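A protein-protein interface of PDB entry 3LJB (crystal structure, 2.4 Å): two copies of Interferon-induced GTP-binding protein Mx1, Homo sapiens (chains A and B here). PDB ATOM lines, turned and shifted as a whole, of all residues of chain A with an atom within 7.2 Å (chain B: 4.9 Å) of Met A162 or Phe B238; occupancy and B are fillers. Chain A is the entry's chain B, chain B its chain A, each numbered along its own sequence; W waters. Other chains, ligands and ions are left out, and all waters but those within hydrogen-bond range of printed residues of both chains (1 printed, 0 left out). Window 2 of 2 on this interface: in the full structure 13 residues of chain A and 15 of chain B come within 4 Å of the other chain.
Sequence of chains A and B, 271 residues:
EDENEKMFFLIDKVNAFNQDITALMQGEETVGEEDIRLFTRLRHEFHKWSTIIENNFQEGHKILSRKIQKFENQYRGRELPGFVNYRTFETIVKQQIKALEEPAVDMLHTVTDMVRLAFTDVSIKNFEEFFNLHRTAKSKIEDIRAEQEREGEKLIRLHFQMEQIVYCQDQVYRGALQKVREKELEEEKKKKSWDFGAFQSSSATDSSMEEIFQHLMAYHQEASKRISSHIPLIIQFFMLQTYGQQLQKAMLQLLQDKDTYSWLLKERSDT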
ATOM      1  N   LEU A 155     -23.756  -7.452  26.994  1.00  0.00           N
ATOM      2  CA  LEU A 155     -23.692  -5.997  26.828  1.00  0.00           C
ATOM      3  C   LEU A 155     -22.894  -5.588  25.586  1.00  0.00           C
ATOM      4  O   LEU A 155     -23.212  -4.589  24.937  1.00  0.00           O
ATOM      5  CB  LEU A 155     -23.112  -5.307  28.080  1.00  0.00           C
ATOM      6  CG  LEU A 155     -24.066  -4.784  29.162  1.00  0.00           C
ATOM      7  CD1 LEU A 155     -25.050  -3.756  28.562  1.00  0.00           C
ATOM      8  CD2 LEU A 155     -24.832  -5.933  29.936  1.00  0.00           C
ATOM      9  N   ILE A 156     -21.857  -6.339  25.258  1.00  0.00           N
ATOM     10  CA  ILE A 156     -21.157  -6.095  24.022  1.00  0.00           C
ATOM     11  C   ILE A 156     -22.163  -6.208  22.871  1.00  0.00           C
ATOM     12  O   ILE A 156     -22.197  -5.361  21.967  1.00  0.00           O
ATOM     13  CB  ILE A 156     -19.969  -7.083  23.787  1.00  0.00           C
ATOM     14  CG1 ILE A 156     -18.797  -6.800  24.740  1.00  0.00           C
ATOM     15  CG2 ILE A 156     -19.474  -7.002  22.341  1.00  0.00           C
ATOM     16  CD1 ILE A 156     -17.675  -7.861  24.686  1.00  0.00           C
ATOM     17  N   ARG A 157     -22.974  -7.254  22.890  1.00  0.00           N
ATOM     18  CA  ARG A 157     -23.836  -7.520  21.755  1.00  0.00           C
ATOM     19  C   ARG A 157     -24.964  -6.487  21.706  1.00  0.00           C
ATOM     20  O   ARG A 157     -25.343  -6.034  20.619  1.00  0.00           O
ATOM     21  CB  ARG A 157     -24.367  -8.954  21.780  1.00  0.00           C
ATOM     22  CG  ARG A 157     -23.307 -10.019  21.471  1.00  0.00           C
ATOM     23  CD  ARG A 157     -23.968 -11.361  21.181  1.00  0.00           C
ATOM     24  NE  ARG A 157     -22.977 -12.435  21.117  1.00  0.00           N
ATOM     25  CZ  ARG A 157     -22.257 -12.737  20.036  1.00  0.00           C
ATOM     26  NH1 ARG A 157     -21.372 -13.729  20.104  1.00  0.00           N
ATOM     27  NH2 ARG A 157     -22.409 -12.053  18.889  1.00  0.00           N
ATOM     28  N   LEU A 158     -25.453  -6.084  22.874  1.00  0.00           N
ATOM     29  CA  LEU A 158     -26.416  -4.962  22.958  1.00  0.00           C
ATOM     30  C   LEU A 158     -25.817  -3.686  22.365  1.00  0.00           C
ATOM     31  O   LEU A 158     -26.423  -3.055  21.525  1.00  0.00           O
ATOM     32  CB  LEU A 158     -26.877  -4.733  24.408  1.00  0.00           C
ATOM     33  CG  LEU A 158     -27.804  -3.543  24.665  1.00  0.00           C
ATOM     34  CD1 LEU A 158     -29.160  -3.717  23.978  1.00  0.00           C
ATOM     35  CD2 LEU A 158     -27.978  -3.329  26.167  1.00  0.00           C
ATOM     36  N   HIS A 159     -24.592  -3.346  22.731  1.00  0.00           N
ATOM     37  CA  HIS A 159     -23.952  -2.187  22.108  1.00  0.00           C
ATOM     38  C   HIS A 159     -23.981  -2.245  20.580  1.00  0.00           C
ATOM     39  O   HIS A 159     -24.336  -1.263  19.924  1.00  0.00           O
ATOM     40  CB  HIS A 159     -22.509  -1.980  22.570  1.00  0.00           C
ATOM     41  CG  HIS A 159     -21.954  -0.671  22.124  1.00  0.00           C
ATOM     42  ND1 HIS A 159     -22.246   0.514  22.763  1.00  0.00           N
ATOM     43  CD2 HIS A 159     -21.207  -0.341  21.049  1.00  0.00           C
ATOM     44  CE1 HIS A 159     -21.672   1.516  22.118  1.00  0.00           C
ATOM     45  NE2 HIS A 159     -21.033   1.023  21.074  1.00  0.00           N
ATOM     46  N   PHE A 160     -23.621  -3.386  19.998  1.00  0.00           N
ATOM     47  CA  PHE A 160     -23.659  -3.484  18.542  1.00  0.00           C
ATOM     48  C   PHE A 160     -25.065  -3.392  17.997  1.00  0.00           C
ATOM     49  O   PHE A 160     -25.258  -2.851  16.934  1.00  0.00           O
ATOM     50  CB  PHE A 160     -22.954  -4.733  18.054  1.00  0.00           C
ATOM     51  CG  PHE A 160     -21.480  -4.590  18.055  1.00  0.00           C
ATOM     52  CD1 PHE A 160     -20.740  -4.964  19.153  1.00  0.00           C
ATOM     53  CD2 PHE A 160     -20.831  -4.013  16.963  1.00  0.00           C
ATOM     54  CE1 PHE A 160     -19.366  -4.815  19.157  1.00  0.00           C
ATOM     55  CE2 PHE A 160     -19.461  -3.856  16.963  1.00  0.00           C
ATOM     56  CZ  PHE A 160     -18.726  -4.259  18.056  1.00  0.00           C
ATOM     57  N   GLN A 161     -26.048  -3.909  18.731  1.00  0.00           N
ATOM     58  CA  GLN A 161     -27.445  -3.679  18.393  1.00  0.00           C
ATOM     59  C   GLN A 161     -27.722  -2.166  18.372  1.00  0.00           C
ATOM     60  O   GLN A 161     -28.326  -1.661  17.440  1.00  0.00           O
ATOM     61  CB  GLN A 161     -28.356  -4.402  19.396  1.00  0.00           C
ATOM     62  CG  GLN A 161     -29.751  -4.691  18.932  1.00  0.00           C
ATOM     63  CD  GLN A 161     -30.637  -5.277  20.042  1.00  0.00           C
ATOM     64  OE1 GLN A 161     -31.861  -5.063  20.059  1.00  0.00           O
ATOM     65  NE2 GLN A 161     -30.032  -6.013  20.968  1.00  0.00           N
ATOM     66  N   MET A 162     -27.244  -1.442  19.380  1.00  0.00           N
ATOM     67  CA  MET A 162     -27.465  -0.005  19.458  1.00  0.00           C
ATOM     68  C   MET A 162     -26.810   0.703  18.298  1.00  0.00           C
ATOM     69  O   MET A 162     -27.394   1.618  17.724  1.00  0.00           O
ATOM     70  CB  MET A 162     -26.911   0.569  20.758  1.00  0.00           C
ATOM     71  CG  MET A 162     -27.624   0.066  21.996  1.00  0.00           C
ATOM     72  SD  MET A 162     -27.276   1.088  23.429  1.00  0.00           S
ATOM     73  CE  MET A 162     -28.091   0.164  24.738  1.00  0.00           C
ATOM     74  N   GLU A 163     -25.597   0.292  17.946  1.00  0.00           N
ATOM     75  CA  GLU A 163     -24.873   0.967  16.867  1.00  0.00           C
ATOM     76  C   GLU A 163     -25.620   0.935  15.534  1.00  0.00           C
ATOM     77  O   GLU A 163     -25.490   1.853  14.725  1.00  0.00           O
ATOM     78  CB  GLU A 163     -23.474   0.377  16.697  1.00  0.00           C
ATOM     79  CG  GLU A 163     -22.521   0.709  17.855  1.00  0.00           C
ATOM     80  CD  GLU A 163     -22.164   2.168  17.894  1.00  0.00           C
ATOM     81  OE1 GLU A 163     -22.319   2.807  16.842  1.00  0.00           O
ATOM     82  OE2 GLU A 163     -21.748   2.670  18.964  1.00  0.00           O
ATOM     83  N   GLN A 164     -26.421  -0.099  15.307  1.00  0.00           N
ATOM     84  CA  GLN A 164     -27.142  -0.228  14.042  1.00  0.00           C
ATOM     85  C   GLN A 164     -28.167   0.906  13.781  1.00  0.00           C
ATOM     86  O   GLN A 164     -28.728   0.943  12.695  1.00  0.00           O
ATOM     87  CB  GLN A 164     -27.782  -1.627  13.908  1.00  0.00           C
ATOM     88  CG  GLN A 164     -26.754  -2.806  13.884  1.00  0.00           C
ATOM     89  CD  GLN A 164     -25.961  -2.933  12.566  1.00  0.00           C
ATOM     90  OE1 GLN A 164     -26.531  -3.266  11.531  1.00  0.00           O
ATOM     91  NE2 GLN A 164     -24.647  -2.687  12.614  1.00  0.00           N
ATOM     92  N   ILE A 165     -28.399   1.826  14.737  1.00  0.00           N
ATOM     93  CA  ILE A 165     -29.036   3.143  14.420  1.00  0.00           C
ATOM     94  C   ILE A 165     -28.024   4.238  14.043  1.00  0.00           C
ATOM     95  O   ILE A 165     -27.044   4.497  14.757  1.00  0.00           O
ATOM     96  CB  ILE A 165     -29.969   3.694  15.539  1.00  0.00           C
ATOM     97  CG1 ILE A 165     -29.186   4.209  16.760  1.00  0.00           C
ATOM     98  CG2 ILE A 165     -30.976   2.652  15.907  1.00  0.00           C
ATOM     99  CD1 ILE A 165     -29.975   4.170  18.075  1.00  0.00           C
ATOM    100  N   VAL A 166     -28.283   4.873  12.907  1.00  0.00           N
ATOM    101  CA  VAL A 166     -27.448   5.967  12.388  1.00  0.00           C
ATOM    102  C   VAL A 166     -28.086   7.317  12.733  1.00  0.00           C
ATOM    103  O   VAL A 166     -28.615   7.493  13.835  1.00  0.00           O
ATOM    104  CB  VAL A 166     -27.228   5.848  10.854  1.00  0.00           C
ATOM    105  CG1 VAL A 166     -28.461   5.283  10.156  1.00  0.00           C
ATOM    106  CG2 VAL A 166     -26.846   7.210  10.253  1.00  0.00           C
ATOM    107  N   TYR A 219     -20.635   8.993  10.105  1.00  0.00           N
ATOM    108  CA  TYR A 219     -21.271   8.024  10.983  1.00  0.00           C
ATOM    109  C   TYR A 219     -20.431   6.747  11.186  1.00  0.00           C
ATOM    110  O   TYR A 219     -20.512   6.125  12.245  1.00  0.00           O
ATOM    111  CB  TYR A 219     -22.654   7.670  10.450  1.00  0.00           C
ATOM    112  CG  TYR A 219     -23.189   6.353  10.953  1.00  0.00           C
ATOM    113  CD1 TYR A 219     -23.505   6.175  12.298  1.00  0.00           C
ATOM    114  CD2 TYR A 219     -23.383   5.289  10.089  1.00  0.00           C
ATOM    115  CE1 TYR A 219     -24.000   4.965  12.761  1.00  0.00           C
ATOM    116  CE2 TYR A 219     -23.883   4.080  10.544  1.00  0.00           C
ATOM    117  CZ  TYR A 219     -24.190   3.924  11.877  1.00  0.00           C
ATOM    118  OH  TYR A 219     -24.689   2.722  12.323  1.00  0.00           O
ATOM    119  N   ARG A 226     -16.825   5.025  19.111  1.00  0.00           N
ATOM    120  CA  ARG A 226     -17.535   4.475  20.276  1.00  0.00           C
ATOM    121  C   ARG A 226     -17.098   3.038  20.554  1.00  0.00           C
ATOM    122  O   ARG A 226     -16.773   2.688  21.683  1.00  0.00           O
ATOM    123  CB  ARG A 226     -19.054   4.525  20.083  1.00  0.00           C
ATOM    124  CG  ARG A 226     -19.649   5.922  20.196  1.00  0.00           C
ATOM    125  CD  ARG A 226     -21.138   5.992  19.792  1.00  0.00           C
ATOM    126  NE  ARG A 226     -21.341   5.727  18.363  1.00  0.00           N
ATOM    127  CZ  ARG A 226     -22.358   6.165  17.624  1.00  0.00           C
ATOM    128  NH1 ARG A 226     -23.317   6.910  18.149  1.00  0.00           N
ATOM    129  NH2 ARG A 226     -22.422   5.858  16.332  1.00  0.00           N
ATOM    130  N   GLN B 148     -39.633   0.289  28.598  1.00  0.00           N
ATOM    131  CA  GLN B 148     -38.376   0.708  27.956  1.00  0.00           C
ATOM    132  C   GLN B 148     -37.594   1.720  28.805  1.00  0.00           C
ATOM    133  O   GLN B 148     -36.344   1.721  28.816  1.00  0.00           O
ATOM    134  CB  GLN B 148     -38.650   1.264  26.556  1.00  0.00           C
ATOM    135  CG  GLN B 148     -39.259   0.214  25.602  1.00  0.00           C
ATOM    136  CD  GLN B 148     -38.402  -1.027  25.500  1.00  0.00           C
ATOM    137  OE1 GLN B 148     -37.180  -0.931  25.517  1.00  0.00           O
ATOM    138  NE2 GLN B 148     -39.030  -2.200  25.388  1.00  0.00           N
ATOM    139  N   GLU B 151     -35.695  -0.004  31.432  1.00  0.00           N
ATOM    140  CA  GLU B 151     -34.527  -0.653  30.839  1.00  0.00           C
ATOM    141  C   GLU B 151     -33.454   0.385  30.518  1.00  0.00           C
ATOM    142  O   GLU B 151     -32.279   0.195  30.827  1.00  0.00           O
ATOM    143  CB  GLU B 151     -34.943  -1.469  29.607  1.00  0.00           C
ATOM    144  CG  GLU B 151     -33.949  -2.538  29.192  1.00  0.00           C
ATOM    145  CD  GLU B 151     -33.574  -3.481  30.349  1.00  0.00           C
ATOM    146  OE1 GLU B 151     -32.348  -3.764  30.511  1.00  0.00           O
ATOM    147  OE2 GLU B 151     -34.501  -3.904  31.100  1.00  0.00           O
ATOM    148  N   GLY B 152     -33.873   1.515  29.960  1.00  0.00           N
ATOM    149  CA  GLY B 152     -32.947   2.615  29.659  1.00  0.00           C
ATOM    150  C   GLY B 152     -32.294   3.160  30.916  1.00  0.00           C
ATOM    151  O   GLY B 152     -31.093   3.413  30.938  1.00  0.00           O
ATOM    152  N   LEU B 155     -29.531   0.798  32.121  1.00  0.00           N
ATOM    153  CA  LEU B 155     -28.309   0.862  31.323  1.00  0.00           C
ATOM    154  C   LEU B 155     -27.562   2.158  31.585  1.00  0.00           C
ATOM    155  O   LEU B 155     -26.333   2.155  31.667  1.00  0.00           O
ATOM    156  CB  LEU B 155     -28.591   0.703  29.822  1.00  0.00           C
ATOM    157  CG  LEU B 155     -28.288  -0.665  29.222  1.00  0.00           C
ATOM    158  CD1 LEU B 155     -26.780  -0.825  28.961  1.00  0.00           C
ATOM    159  CD2 LEU B 155     -28.807  -1.829  30.108  1.00  0.00           C
ATOM    160  N   HIS B 230     -22.670   8.402  24.832  1.00  0.00           N
ATOM    161  CA  HIS B 230     -23.351   7.131  25.075  1.00  0.00           C
ATOM    162  C   HIS B 230     -24.717   7.254  25.751  1.00  0.00           C
ATOM    163  O   HIS B 230     -25.594   6.412  25.530  1.00  0.00           O
ATOM    164  CB  HIS B 230     -22.477   6.193  25.890  1.00  0.00           C
ATOM    165  CG  HIS B 230     -22.945   4.772  25.856  1.00  0.00           C
ATOM    166  ND1 HIS B 230     -23.107   4.080  24.679  1.00  0.00           N
ATOM    167  CD2 HIS B 230     -23.284   3.916  26.848  1.00  0.00           C
ATOM    168  CE1 HIS B 230     -23.535   2.860  24.944  1.00  0.00           C
ATOM    169  NE2 HIS B 230     -23.645   2.733  26.254  1.00  0.00           N
ATOM    170  N   LEU B 233     -27.289   8.002  23.038  1.00  0.00           N
ATOM    171  CA  LEU B 233     -27.417   6.756  22.300  1.00  0.00           C
ATOM    172  C   LEU B 233     -28.337   5.773  23.028  1.00  0.00           C
ATOM    173  O   LEU B 233     -29.209   5.159  22.422  1.00  0.00           O
ATOM    174  CB  LEU B 233     -26.038   6.135  22.102  1.00  0.00           C
ATOM    175  CG  LEU B 233     -25.990   4.851  21.288  1.00  0.00           C
ATOM    176  CD1 LEU B 233     -26.604   5.094  19.913  1.00  0.00           C
ATOM    177  CD2 LEU B 233     -24.577   4.343  21.185  1.00  0.00           C
ATOM    178  N   ILE B 234     -28.142   5.622  24.330  1.00  0.00           N
ATOM    179  CA  ILE B 234     -28.990   4.735  25.129  1.00  0.00           C
ATOM    180  C   ILE B 234     -30.430   5.215  25.067  1.00  0.00           C
ATOM    181  O   ILE B 234     -31.339   4.451  24.785  1.00  0.00           O
ATOM    182  CB  ILE B 234     -28.497   4.649  26.612  1.00  0.00           C
ATOM    183  CG1 ILE B 234     -27.192   3.841  26.690  1.00  0.00           C
ATOM    184  CG2 ILE B 234     -29.578   4.027  27.528  1.00  0.00           C
ATOM    185  CD1 ILE B 234     -26.412   4.063  28.008  1.00  0.00           C
ATOM    186  N   ILE B 235     -30.627   6.495  25.321  1.00  0.00           N
ATOM    187  CA  ILE B 235     -31.967   7.078  25.348  1.00  0.00           C
ATOM    188  C   ILE B 235     -32.727   6.919  24.000  1.00  0.00           C
ATOM    189  O   ILE B 235     -33.877   6.505  23.943  1.00  0.00           O
ATOM    190  CB  ILE B 235     -31.852   8.557  25.752  1.00  0.00           C
ATOM    191  CG1 ILE B 235     -31.508   8.646  27.251  1.00  0.00           C
ATOM    192  CG2 ILE B 235     -33.148   9.321  25.452  1.00  0.00           C
ATOM    193  CD1 ILE B 235     -31.053  10.020  27.712  1.00  0.00           C
ATOM    194  N   GLN B 236     -32.050   7.265  22.918  1.00  0.00           N
ATOM    195  CA  GLN B 236     -32.612   7.197  21.604  1.00  0.00           C
ATOM    196  C   GLN B 236     -32.939   5.739  21.218  1.00  0.00           C
ATOM    197  O   GLN B 236     -34.003   5.467  20.671  1.00  0.00           O
ATOM    198  CB  GLN B 236     -31.596   7.822  20.681  1.00  0.00           C
ATOM    199  CG  GLN B 236     -31.934   7.907  19.229  1.00  0.00           C
ATOM    200  CD  GLN B 236     -30.936   8.817  18.526  1.00  0.00           C
ATOM    201  OE1 GLN B 236     -30.144   8.380  17.692  1.00  0.00           O
ATOM    202  NE2 GLN B 236     -30.946  10.083  18.905  1.00  0.00           N
ATOM    203  N   PHE B 237     -32.047   4.798  21.538  1.00  0.00           N
ATOM    204  CA  PHE B 237     -32.257   3.401  21.198  1.00  0.00           C
ATOM    205  C   PHE B 237     -33.458   2.831  21.895  1.00  0.00           C
ATOM    206  O   PHE B 237     -34.222   2.087  21.282  1.00  0.00           O
ATOM    207  CB  PHE B 237     -31.030   2.549  21.559  1.00  0.00           C
ATOM    208  CG  PHE B 237     -31.278   1.054  21.480  1.00  0.00           C
ATOM    209  CD1 PHE B 237     -31.259   0.395  20.264  1.00  0.00           C
ATOM    210  CD2 PHE B 237     -31.531   0.317  22.621  1.00  0.00           C
ATOM    211  CE1 PHE B 237     -31.488  -0.975  20.192  1.00  0.00           C
ATOM    212  CE2 PHE B 237     -31.767  -1.058  22.552  1.00  0.00           C
ATOM    213  CZ  PHE B 237     -31.757  -1.699  21.349  1.00  0.00           C
ATOM    214  N   PHE B 238     -33.597   3.125  23.186  1.00  0.00           N
ATOM    215  CA  PHE B 238     -34.665   2.556  23.982  1.00  0.00           C
ATOM    216  C   PHE B 238     -35.964   3.305  23.812  1.00  0.00           C
ATOM    217  O   PHE B 238     -37.011   2.675  23.649  1.00  0.00           O
ATOM    218  CB  PHE B 238     -34.297   2.489  25.475  1.00  0.00           C
ATOM    219  CG  PHE B 238     -33.449   1.306  25.834  1.00  0.00           C
ATOM    220  CD1 PHE B 238     -33.982   0.018  25.786  1.00  0.00           C
ATOM    221  CD2 PHE B 238     -32.119   1.466  26.187  1.00  0.00           C
ATOM    222  CE1 PHE B 238     -33.188  -1.098  26.091  1.00  0.00           C
ATOM    223  CE2 PHE B 238     -31.327   0.369  26.507  1.00  0.00           C
ATOM    224  CZ  PHE B 238     -31.862  -0.921  26.449  1.00  0.00           C
ATOM    225  N   MET B 239     -35.907   4.636  23.847  1.00  0.00           N
ATOM    226  CA  MET B 239     -37.112   5.448  23.949  1.00  0.00           C
ATOM    227  C   MET B 239     -37.571   6.106  22.659  1.00  0.00           C
ATOM    228  O   MET B 239     -38.582   6.803  22.674  1.00  0.00           O
ATOM    229  CB  MET B 239     -36.929   6.537  25.007  1.00  0.00           C
ATOM    230  CG  MET B 239     -36.318   6.060  26.327  1.00  0.00           C
ATOM    231  SD  MET B 239     -37.170   4.643  27.032  1.00  0.00           S
ATOM    232  CE  MET B 239     -38.888   5.159  26.937  1.00  0.00           C
ATOM    233  N   LEU B 240     -36.857   5.907  21.550  1.00  0.00           N
ATOM    234  CA  LEU B 240     -37.436   6.232  20.250  1.00  0.00           C
ATOM    235  C   LEU B 240     -37.407   5.019  19.345  1.00  0.00           C
ATOM    236  O   LEU B 240     -38.453   4.524  18.966  1.00  0.00           O
ATOM    237  CB  LEU B 240     -36.767   7.438  19.587  1.00  0.00           C
ATOM    238  CG  LEU B 240     -37.381   7.835  18.229  1.00  0.00           C
ATOM    239  CD1 LEU B 240     -38.822   8.282  18.395  1.00  0.00           C
ATOM    240  CD2 LEU B 240     -36.537   8.899  17.539  1.00  0.00           C
ATOM    241  N   THR B 242     -36.580   1.605  19.866  1.00  0.00           N
ATOM    242  CA  THR B 242     -37.190   0.365  20.384  1.00  0.00           C
ATOM    243  C   THR B 242     -38.655   0.607  20.736  1.00  0.00           C
ATOM    244  O   THR B 242     -39.528  -0.166  20.359  1.00  0.00           O
ATOM    245  CB  THR B 242     -36.433  -0.199  21.623  1.00  0.00           C
ATOM    246  OG1 THR B 242     -35.070  -0.447  21.266  1.00  0.00           O
ATOM    247  CG2 THR B 242     -37.066  -1.496  22.142  1.00  0.00           C
ATOM    248  N   TYR B 243     -38.913   1.688  21.458  1.00  0.00           N
ATOM    249  CA  TYR B 243     -40.279   2.121  21.797  1.00  0.00           C
ATOM    250  C   TYR B 243     -41.172   2.133  20.551  1.00  0.00           C
ATOM    251  O   TYR B 243     -42.267   1.528  20.522  1.00  0.00           O
ATOM    252  CB  TYR B 243     -40.212   3.509  22.439  1.00  0.00           C
ATOM    253  CG  TYR B 243     -41.470   4.064  23.085  1.00  0.00           C
ATOM    254  CD1 TYR B 243     -42.655   3.344  23.164  1.00  0.00           C
ATOM    255  CD2 TYR B 243     -41.447   5.320  23.635  1.00  0.00           C
ATOM    256  CE1 TYR B 243     -43.786   3.892  23.763  1.00  0.00           C
ATOM    257  CE2 TYR B 243     -42.559   5.873  24.224  1.00  0.00           C
ATOM    258  CZ  TYR B 243     -43.722   5.160  24.297  1.00  0.00           C
ATOM    259  OH  TYR B 243     -44.822   5.735  24.912  1.00  0.00           O
HETATM  260  O   HOH W   1     -22.898   0.037  25.360  1.00  0.00           O
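O of Phe B237 sits at hydrogen-bond distance from OG1 of Thr B242, 2.7 Å away.
NH2 of Arg A226 is in salt-bridge range of OE1 of Glu A163.
N of Tyr B243 lies within hydrogen-bond range of O of Phe B238.
A ring nitrogen (NE2) of His A159 sits at hydrogen-bond distance from the side-chain carboxylate of Glu A163 (2.8 Å).
O of Glu A163 sits at hydrogen-bond distance from OH of Tyr A219.
Leu B155 touches Leu A155 (CD1 to CD1, 3.4 Å).
Leu A158 touches Leu B155 (CD2 to CD1, 3.9 Å).
CD1 of Leu A158 touches CE2 of Phe B237, 3.99 Å away.
ND1 of His A159 touches CE1 of His B230, 3.5 Å away.
CZ of Phe B237 touches OE1 of Gln A161, at 3.6 Å.
Met A162 touches Phe B237 (CG to CG, 3.8 Å).
CE of Met A162 touches CE2 of Phe B238, 3.7 Å away.
Glu A163 touches Leu B233 (OE2 to CD2, 3.97 Å).
Ile A165 touches Leu B233 (CD1 to CD1, 3.9 Å).
CD1 of Ile A165 touches CA of Phe B237, 3.9 Å away.
Of the printed residues of chain B, Leu A155 touches Leu B155 (3.4 Å).
Printed residues of chain B within 4 Å of Gln A161: Phe B237 (3.6 Å).
Met A162 touches just these residues of chain B: Phe B237 and Phe B238.
Printed residues of chain B within 4 Å of Glu A163: Leu B233 (3.97 Å).
Gly B152 touches none of the printed residues of chain A.
Of the printed residues of chain A, Leu B233 touches Glu A163 (3.97 Å) and Ile A165 (3.9 Å).
Phe B238 touches just one residue of chain A: Met A162.
Hydrophobic or aromatic side chains of chain B within 4 Å of the printed part of chain A: Leu B155, His B230, Leu B233, Phe B237 and Phe B238.
Along chain B the printed residues that touch a printed residue of chain A span positions 155 to 238.
Hydrophobic or aromatic side chains of chain A within 4 Å of the printed part of chain B: Leu A155, Leu A158, His A159, Met A162 and Ile A165.
Among the printed residues, no Asp or Glu carboxylate lies within 4 Å of a Lys or Arg side-chain nitrogen of the other chain.
Leu A155 touches its own counterpart, Leu B155.
Position printed for both chains: 155.
Of the 10 pairs that touch across the chains among the printed residues, 1 has its exchanged pair printed and touching as well.
Water W1 lies within hydrogen-bond range of ND1 of His A159 and NE2 of His B230.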
